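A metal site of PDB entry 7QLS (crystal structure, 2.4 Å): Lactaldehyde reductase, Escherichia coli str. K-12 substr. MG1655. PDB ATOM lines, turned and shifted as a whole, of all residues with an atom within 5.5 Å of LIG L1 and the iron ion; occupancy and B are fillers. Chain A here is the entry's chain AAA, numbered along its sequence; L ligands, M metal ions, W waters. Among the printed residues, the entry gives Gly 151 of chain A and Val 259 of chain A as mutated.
The side-chain amide nitrogen (ND2) of Asn 281 sits close to the side-chain carboxylate (OD1) of Asp 196 (2.8 Å). The side-chain amide nitrogen (ND2) of Asn 281 sits close to a ring nitrogen (NE2) of His 263 (3.4 Å). The side-chain hydroxyl (OG) of Ser 255 lies within hydrogen-bond range of the backbone NH (N) of Ile 150 (3.0 Å). The side-chain amide nitrogen (ND2) of Asn 281 sits close to a ring nitrogen (NE2) of His 277, 3.1 Å away.
Merely in contact with LIG L1: Thr 144 (3.8 Å), Thr 149 (3.9 Å), Gly 151 (3.5 Å), Val 153 (3.7 Å), Phe 254 (3.2 Å), Ser 255 (3.5 Å), Val 259 (3.6 Å) and Cys 362 (3.4 Å). 11 residues have an atom within 4 Å of LIG L1: Thr 144, Thr 149, Gly 151, Val 153, His 200, Phe 254, Ser 255, Val 259, His 263, His 277 and Cys 362.
Merely in contact with the iron ion: Asn 281 (3.7 Å). Five residues have an atom within 4 Å of the iron ion: Asp 196, His 200, His 263, His 277 and Asn 281.
The iron ion is bound by a ring nitrogen (NE2) of His 277, a ring nitrogen (NE2) of His 263, water W2, a ring nitrogen (NE2) of His 200, the side-chain carboxylate (OD1) of Asp 196 and an oxygen (O2) of LIG L1. The iron ion has six donor atoms within binding distance.
Water W2 lies within hydrogen-bond range of the side-chain carboxylate (OD2) of Asp 196 (2.5 Å), an oxygen (O12) of LG2 L2 (3.0 Å) and a nitrogen (N1) of LIG L1 (3.5 Å). Water W1 lies within hydrogen-bond range of a nitrogen (N1) of LIG L1 (2.6 Å), the backbone carbonyl oxygen of Thr 144 (3.0 Å) and the side-chain hydroxyl of Thr 149 (3.1 Å). Water W3 lies within hydrogen-bond range of O13 of LG2 L2 (2.7 Å) and NE2 of His 267 (2.9 Å).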
ATOM      1  N   THR A 144      29.785   8.512  16.652  1.00  0.00           N
ATOM      2  CA  THR A 144      28.571   9.334  16.432  1.00  0.00           C
ATOM      3  C   THR A 144      27.606   9.229  17.605  1.00  0.00           C
ATOM      4  O   THR A 144      26.788  10.130  17.760  1.00  0.00           O
ATOM      5  CB  THR A 144      27.836   8.988  15.125  1.00  0.00           C
ATOM      6  OG1 THR A 144      27.273   7.681  15.266  1.00  0.00           O
ATOM      7  CG2 THR A 144      28.751   9.039  13.920  1.00  0.00           C
ATOM      8  N   THR A 149      21.299   8.369  20.654  1.00  0.00           N
ATOM      9  CA  THR A 149      20.665   9.678  20.294  1.00  0.00           C
ATOM     10  C   THR A 149      19.323   9.437  19.591  1.00  0.00           C
ATOM     11  O   THR A 149      19.163   8.343  19.009  1.00  0.00           O
ATOM     12  CB  THR A 149      21.604  10.531  19.437  1.00  0.00           C
ATOM     13  OG1 THR A 149      21.696   9.920  18.144  1.00  0.00           O
ATOM     14  CG2 THR A 149      22.978  10.708  20.038  1.00  0.00           C
ATOM     15  N   ILE A 150      18.404  10.414  19.640  1.00  0.00           N
ATOM     16  CA  ILE A 150      17.071  10.371  18.966  1.00  0.00           C
ATOM     17  C   ILE A 150      17.143  11.071  17.599  1.00  0.00           C
ATOM     18  O   ILE A 150      16.075  11.399  17.048  1.00  0.00           O
ATOM     19  CB  ILE A 150      15.941  10.972  19.842  1.00  0.00           C
ATOM     20  CG1 ILE A 150      16.216  12.433  20.218  1.00  0.00           C
ATOM     21  CG2 ILE A 150      15.712  10.102  21.070  1.00  0.00           C
ATOM     22  CD1 ILE A 150      14.991  13.181  20.695  1.00  0.00           C
ATOM     23  N   GLY A 151      18.357  11.252  17.064  1.00  0.00           N
ATOM     24  CA  GLY A 151      18.617  11.938  15.784  1.00  0.00           C
ATOM     25  C   GLY A 151      19.208  11.000  14.738  1.00  0.00           C
ATOM     26  O   GLY A 151      19.896  10.011  15.121  1.00  0.00           O
ATOM     27  N   TYR A 152      18.957  11.281  13.455  1.00  0.00           N
ATOM     28  CA  TYR A 152      19.644  10.664  12.304  1.00  0.00           C
ATOM     29  C   TYR A 152      19.718  11.672  11.155  1.00  0.00           C
ATOM     30  O   TYR A 152      18.800  12.514  11.009  1.00  0.00           O
ATOM     31  CB  TYR A 152      18.980   9.336  11.900  1.00  0.00           C
ATOM     32  CG  TYR A 152      17.496   9.360  11.624  1.00  0.00           C
ATOM     33  CD1 TYR A 152      16.573   9.445  12.654  1.00  0.00           C
ATOM     34  CD2 TYR A 152      17.007   9.209  10.338  1.00  0.00           C
ATOM     35  CE1 TYR A 152      15.208   9.422  12.409  1.00  0.00           C
ATOM     36  CE2 TYR A 152      15.646   9.186  10.069  1.00  0.00           C
ATOM     37  CZ  TYR A 152      14.742   9.296  11.106  1.00  0.00           C
ATOM     38  OH  TYR A 152      13.406   9.280  10.858  1.00  0.00           O
ATOM     39  N   VAL A 153      20.801  11.608  10.381  1.00  0.00           N
ATOM     40  CA  VAL A 153      21.125  12.611   9.333  1.00  0.00           C
ATOM     41  C   VAL A 153      21.182  11.895   7.973  1.00  0.00           C
ATOM     42  O   VAL A 153      22.026  10.988   7.793  1.00  0.00           O
ATOM     43  CB  VAL A 153      22.427  13.372   9.672  1.00  0.00           C
ATOM     44  CG1 VAL A 153      22.699  14.484   8.694  1.00  0.00           C
ATOM     45  CG2 VAL A 153      22.370  13.916  11.083  1.00  0.00           C
ATOM     46  N   VAL A 164      18.470  16.794   9.327  1.00  0.00           N
ATOM     47  CA  VAL A 164      18.410  16.117  10.651  1.00  0.00           C
ATOM     48  C   VAL A 164      16.952  15.773  10.967  1.00  0.00           C
ATOM     49  O   VAL A 164      16.088  16.670  10.867  1.00  0.00           O
ATOM     50  CB  VAL A 164      19.048  16.995  11.730  1.00  0.00           C
ATOM     51  CG1 VAL A 164      19.063  16.299  13.086  1.00  0.00           C
ATOM     52  CG2 VAL A 164      20.451  17.434  11.326  1.00  0.00           C
ATOM     53  N   VAL A 166      14.584  14.186  14.097  1.00  0.00           N
ATOM     54  CA  VAL A 166      14.632  14.071  15.583  1.00  0.00           C
ATOM     55  C   VAL A 166      13.304  13.468  16.053  1.00  0.00           C
ATOM     56  O   VAL A 166      12.241  14.048  15.766  1.00  0.00           O
ATOM     57  CB  VAL A 166      14.903  15.448  16.244  1.00  0.00           C
ATOM     58  CG1 VAL A 166      14.909  15.349  17.762  1.00  0.00           C
ATOM     59  CG2 VAL A 166      16.206  16.050  15.746  1.00  0.00           C
ATOM     60  N   ASP A 196      34.705  13.900  16.396  1.00  0.00           N
ATOM     61  CA  ASP A 196      33.236  14.070  16.262  1.00  0.00           C
ATOM     62  C   ASP A 196      32.619  13.907  17.659  1.00  0.00           C
ATOM     63  O   ASP A 196      31.789  14.759  18.048  1.00  0.00           O
ATOM     64  CB  ASP A 196      32.664  13.138  15.190  1.00  0.00           C
ATOM     65  CG  ASP A 196      31.144  13.167  15.049  1.00  0.00           C
ATOM     66  OD1 ASP A 196      30.560  14.263  15.124  1.00  0.00           O
ATOM     67  OD2 ASP A 196      30.568  12.082  14.840  1.00  0.00           O
ATOM     68  N   HIS A 200      30.669  16.815  19.903  1.00  0.00           N
ATOM     69  CA  HIS A 200      29.368  16.551  20.566  1.00  0.00           C
ATOM     70  C   HIS A 200      29.437  16.974  22.029  1.00  0.00           C
ATOM     71  O   HIS A 200      28.495  17.613  22.513  1.00  0.00           O
ATOM     72  CB  HIS A 200      29.004  15.060  20.490  1.00  0.00           C
ATOM     73  CG  HIS A 200      28.679  14.603  19.119  1.00  0.00           C
ATOM     74  ND1 HIS A 200      28.951  13.328  18.707  1.00  0.00           N
ATOM     75  CD2 HIS A 200      28.116  15.244  18.075  1.00  0.00           C
ATOM     76  CE1 HIS A 200      28.558  13.188  17.453  1.00  0.00           C
ATOM     77  NE2 HIS A 200      28.045  14.351  17.043  1.00  0.00           N
ATOM     78  N   PHE A 254      24.007  15.307  24.420  1.00  0.00           N
ATOM     79  CA  PHE A 254      23.744  16.290  23.334  1.00  0.00           C
ATOM     80  C   PHE A 254      22.415  15.958  22.667  1.00  0.00           C
ATOM     81  O   PHE A 254      21.686  16.899  22.331  1.00  0.00           O
ATOM     82  CB  PHE A 254      24.917  16.355  22.355  1.00  0.00           C
ATOM     83  CG  PHE A 254      24.960  15.305  21.275  1.00  0.00           C
ATOM     84  CD1 PHE A 254      24.224  15.445  20.115  1.00  0.00           C
ATOM     85  CD2 PHE A 254      25.810  14.217  21.386  1.00  0.00           C
ATOM     86  CE1 PHE A 254      24.295  14.507  19.105  1.00  0.00           C
ATOM     87  CE2 PHE A 254      25.888  13.273  20.373  1.00  0.00           C
ATOM     88  CZ  PHE A 254      25.120  13.412  19.233  1.00  0.00           C
ATOM     89  N   SER A 255      22.088  14.665  22.526  1.00  0.00           N
ATOM     90  CA  SER A 255      20.789  14.174  21.995  1.00  0.00           C
ATOM     91  C   SER A 255      19.628  14.939  22.651  1.00  0.00           C
ATOM     92  O   SER A 255      18.668  15.282  21.952  1.00  0.00           O
ATOM     93  CB  SER A 255      20.650  12.679  22.227  1.00  0.00           C
ATOM     94  OG  SER A 255      19.344  12.208  21.919  1.00  0.00           O
ATOM     95  N   GLY A 258      21.049  19.486  22.628  1.00  0.00           N
ATOM     96  CA  GLY A 258      21.483  20.029  21.330  1.00  0.00           C
ATOM     97  C   GLY A 258      22.996  20.194  21.225  1.00  0.00           C
ATOM     98  O   GLY A 258      23.704  19.912  22.195  1.00  0.00           O
ATOM     99  N   VAL A 259      23.456  20.647  20.064  1.00  0.00           N
ATOM    100  CA  VAL A 259      24.875  20.978  19.770  1.00  0.00           C
ATOM    101  C   VAL A 259      24.907  22.454  19.316  1.00  0.00           C
ATOM    102  O   VAL A 259      24.320  23.297  20.035  1.00  0.00           O
ATOM    103  CB  VAL A 259      25.465  19.982  18.758  1.00  0.00           C
ATOM    104  CG1 VAL A 259      25.824  18.664  19.422  1.00  0.00           C
ATOM    105  CG2 VAL A 259      24.548  19.745  17.580  1.00  0.00           C
ATOM    106  N   HIS A 263      28.517  21.559  13.983  1.00  0.00           N
ATOM    107  CA  HIS A 263      27.657  20.571  13.267  1.00  0.00           C
ATOM    108  C   HIS A 263      26.872  21.276  12.155  1.00  0.00           C
ATOM    109  O   HIS A 263      26.716  20.668  11.080  1.00  0.00           O
ATOM    110  CB  HIS A 263      26.769  19.826  14.268  1.00  0.00           C
ATOM    111  CG  HIS A 263      27.418  18.594  14.794  1.00  0.00           C
ATOM    112  ND1 HIS A 263      28.492  18.639  15.659  1.00  0.00           N
ATOM    113  CD2 HIS A 263      27.195  17.293  14.537  1.00  0.00           C
ATOM    114  CE1 HIS A 263      28.880  17.411  15.922  1.00  0.00           C
ATOM    115  NE2 HIS A 263      28.099  16.566  15.254  1.00  0.00           N
ATOM    116  N   HIS A 267      27.675  19.947   8.203  1.00  0.00           N
ATOM    117  CA  HIS A 267      26.651  19.228   7.398  1.00  0.00           C
ATOM    118  C   HIS A 267      26.706  19.660   5.938  1.00  0.00           C
ATOM    119  O   HIS A 267      26.681  18.806   5.062  1.00  0.00           O
ATOM    120  CB  HIS A 267      25.250  19.369   8.027  1.00  0.00           C
ATOM    121  CG  HIS A 267      25.076  18.542   9.255  1.00  0.00           C
ATOM    122  ND1 HIS A 267      23.934  18.627  10.036  1.00  0.00           N
ATOM    123  CD2 HIS A 267      25.882  17.619   9.833  1.00  0.00           C
ATOM    124  CE1 HIS A 267      24.053  17.787  11.045  1.00  0.00           C
ATOM    125  NE2 HIS A 267      25.250  17.163  10.948  1.00  0.00           N
ATOM    126  N   HIS A 277      32.239  13.479   8.170  1.00  0.00           N
ATOM    127  CA  HIS A 277      31.614  14.306   9.231  1.00  0.00           C
ATOM    128  C   HIS A 277      32.638  14.692  10.318  1.00  0.00           C
ATOM    129  O   HIS A 277      32.665  15.871  10.722  1.00  0.00           O
ATOM    130  CB  HIS A 277      30.409  13.536   9.794  1.00  0.00           C
ATOM    131  CG  HIS A 277      29.741  14.195  10.952  1.00  0.00           C
ATOM    132  ND1 HIS A 277      29.026  15.376  10.825  1.00  0.00           N
ATOM    133  CD2 HIS A 277      29.629  13.828  12.242  1.00  0.00           C
ATOM    134  CE1 HIS A 277      28.523  15.707  11.981  1.00  0.00           C
ATOM    135  NE2 HIS A 277      28.872  14.766  12.873  1.00  0.00           N
ATOM    136  N   ASN A 281      34.036  18.515  11.256  1.00  0.00           N
ATOM    137  CA  ASN A 281      33.847  18.938  12.675  1.00  0.00           C
ATOM    138  C   ASN A 281      35.198  19.339  13.272  1.00  0.00           C
ATOM    139  O   ASN A 281      35.233  20.376  13.934  1.00  0.00           O
ATOM    140  CB  ASN A 281      33.219  17.850  13.540  1.00  0.00           C
ATOM    141  CG  ASN A 281      31.706  17.805  13.422  1.00  0.00           C
ATOM    142  OD1 ASN A 281      31.078  18.772  13.031  1.00  0.00           O
ATOM    143  ND2 ASN A 281      31.111  16.678  13.759  1.00  0.00           N
ATOM    144  N   VAL A 361      19.357  22.715  11.414  1.00  0.00           N
ATOM    145  CA  VAL A 361      18.688  22.555  12.732  1.00  0.00           C
ATOM    146  C   VAL A 361      19.689  22.831  13.861  1.00  0.00           C
ATOM    147  O   VAL A 361      19.305  23.471  14.857  1.00  0.00           O
ATOM    148  CB  VAL A 361      18.070  21.148  12.881  1.00  0.00           C
ATOM    149  CG1 VAL A 361      17.662  20.827  14.314  1.00  0.00           C
ATOM    150  CG2 VAL A 361      16.888  20.918  11.934  1.00  0.00           C
ATOM    151  N   CYS A 362      20.928  22.341  13.729  1.00  0.00           N
ATOM    152  CA  CYS A 362      21.972  22.341  14.804  1.00  0.00           C
ATOM    153  C   CYS A 362      22.311  23.765  15.248  1.00  0.00           C
ATOM    154  O   CYS A 362      22.670  23.943  16.439  1.00  0.00           O
ATOM    155  CB  CYS A 362      23.223  21.623  14.340  1.00  0.00           C
ATOM    156  SG  CYS A 362      22.955  19.851  14.052  1.00  0.00           S
HETATM  157  N1  LIG L   1      25.036  12.976  16.023  1.00  0.00           N
HETATM  158  C1  LIG L   1      22.190  17.343  16.223  1.00  0.00           C
HETATM  159  C2  LIG L   1      25.011  13.937  15.111  1.00  0.00           C
HETATM  160  C3  LIG L   1      20.040  13.955  18.575  1.00  0.00           C
HETATM  161  O1  LIG L   1      19.823  15.005  17.629  1.00  0.00           O
HETATM  162  C4  LIG L   1      22.780  15.136  15.426  1.00  0.00           C
HETATM  163  C5  LIG L   1      23.010  16.504  15.473  1.00  0.00           C
HETATM  164  C6  LIG L   1      21.137  16.807  16.934  1.00  0.00           C
HETATM  165  C7  LIG L   1      20.904  15.421  16.911  1.00  0.00           C
HETATM  166  C8  LIG L   1      21.738  14.600  16.163  1.00  0.00           C
HETATM  167  O2  LIG L   1      26.022  14.544  14.741  1.00  0.00           O
HETATM  168  C9  LIG L   1      23.611  14.244  14.530  1.00  0.00           C
HETATM  169  O3  LIG L   1      20.262  17.545  17.692  1.00  0.00           O
HETATM  170  C10 LIG L   1      19.607  18.636  17.066  1.00  0.00           C
HETATM  171  N1  LG2 L   2      36.468  -0.931  10.571  1.00  0.00           N
HETATM  172  C1  LG2 L   2      36.682  -0.541   9.310  1.00  0.00           C
HETATM  173  N2  LG2 L   2      36.037   0.365   8.579  1.00  0.00           N
HETATM  174  C2  LG2 L   2      35.030   0.905   9.280  1.00  0.00           C
HETATM  175  C3  LG2 L   2      34.677   0.608  10.577  1.00  0.00           C
HETATM  176  C4  LG2 L   2      35.440  -0.356  11.257  1.00  0.00           C
HETATM  177  N3  LG2 L   2      35.228  -0.740  12.510  1.00  0.00           N
HETATM  178  N4  LG2 L   2      33.587   1.379  10.963  1.00  0.00           N
HETATM  179  C5  LG2 L   2      33.301   2.112   9.908  1.00  0.00           C
HETATM  180  N5  LG2 L   2      34.150   1.862   8.851  1.00  0.00           N
HETATM  181  C6  LG2 L   2      34.146   2.501   7.530  1.00  0.00           C
HETATM  182  C7  LG2 L   2      32.805   2.451   6.814  1.00  0.00           C
HETATM  183  O1  LG2 L   2      32.667   1.224   6.128  1.00  0.00           O
HETATM  184  C8  LG2 L   2      32.933   3.649   5.867  1.00  0.00           C
HETATM  185  O2  LG2 L   2      33.626   3.274   4.691  1.00  0.00           O
HETATM  186  O3  LG2 L   2      34.436   3.873   7.698  1.00  0.00           O
HETATM  187  C9  LG2 L   2      33.738   4.659   6.703  1.00  0.00           C
HETATM  188  C10 LG2 L   2      32.932   5.740   7.380  1.00  0.00           C
HETATM  189  O4  LG2 L   2      31.785   5.153   8.067  1.00  0.00           O
HETATM  190  P1  LG2 L   2      30.614   6.072   8.647  1.00  0.00           P
HETATM  191  O5  LG2 L   2      29.524   5.203   9.191  1.00  0.00           O
HETATM  192  O6  LG2 L   2      30.255   7.126   7.649  1.00  0.00           O
HETATM  193  O7  LG2 L   2      31.340   6.782   9.901  1.00  0.00           O
HETATM  194  P2  LG2 L   2      30.771   7.700  11.082  1.00  0.00           P
HETATM  195  O8  LG2 L   2      30.500   6.833  12.258  1.00  0.00           O
HETATM  196  O9  LG2 L   2      31.679   8.880  11.252  1.00  0.00           O
HETATM  197  O10 LG2 L   2      29.380   8.192  10.484  1.00  0.00           O
HETATM  198  C11 LG2 L   2      29.125   9.601  10.279  1.00  0.00           C
HETATM  199  O11 LG2 L   2      26.845   9.877  10.994  1.00  0.00           O
HETATM  200  O12 LG2 L   2      26.175  11.664  12.297  1.00  0.00           O
HETATM  201  C12 LG2 L   2      26.176  11.136  11.014  1.00  0.00           C
HETATM  202  O13 LG2 L   2      26.223  13.099   9.477  1.00  0.00           O
HETATM  203  C13 LG2 L   2      26.952  12.022  10.036  1.00  0.00           C
HETATM  204  O14 LG2 L   2      26.420  10.711   7.988  1.00  0.00           O
HETATM  205  C14 LG2 L   2      27.408  11.008   8.970  1.00  0.00           C
HETATM  206  C15 LG2 L   2      27.696   9.775   9.833  1.00  0.00           C
HETATM  207 FE    FE M   1      28.358  14.499  14.885  1.00  0.00          FE
HETATM  208  O   HOH W   1      24.155  10.584  16.453  1.00  0.00           O
HETATM  209  O   HOH W   2      28.097  12.397  14.513  1.00  0.00           O
HETATM  210  O   HOH W   3      25.703  14.458  11.788  1.00  0.00           O
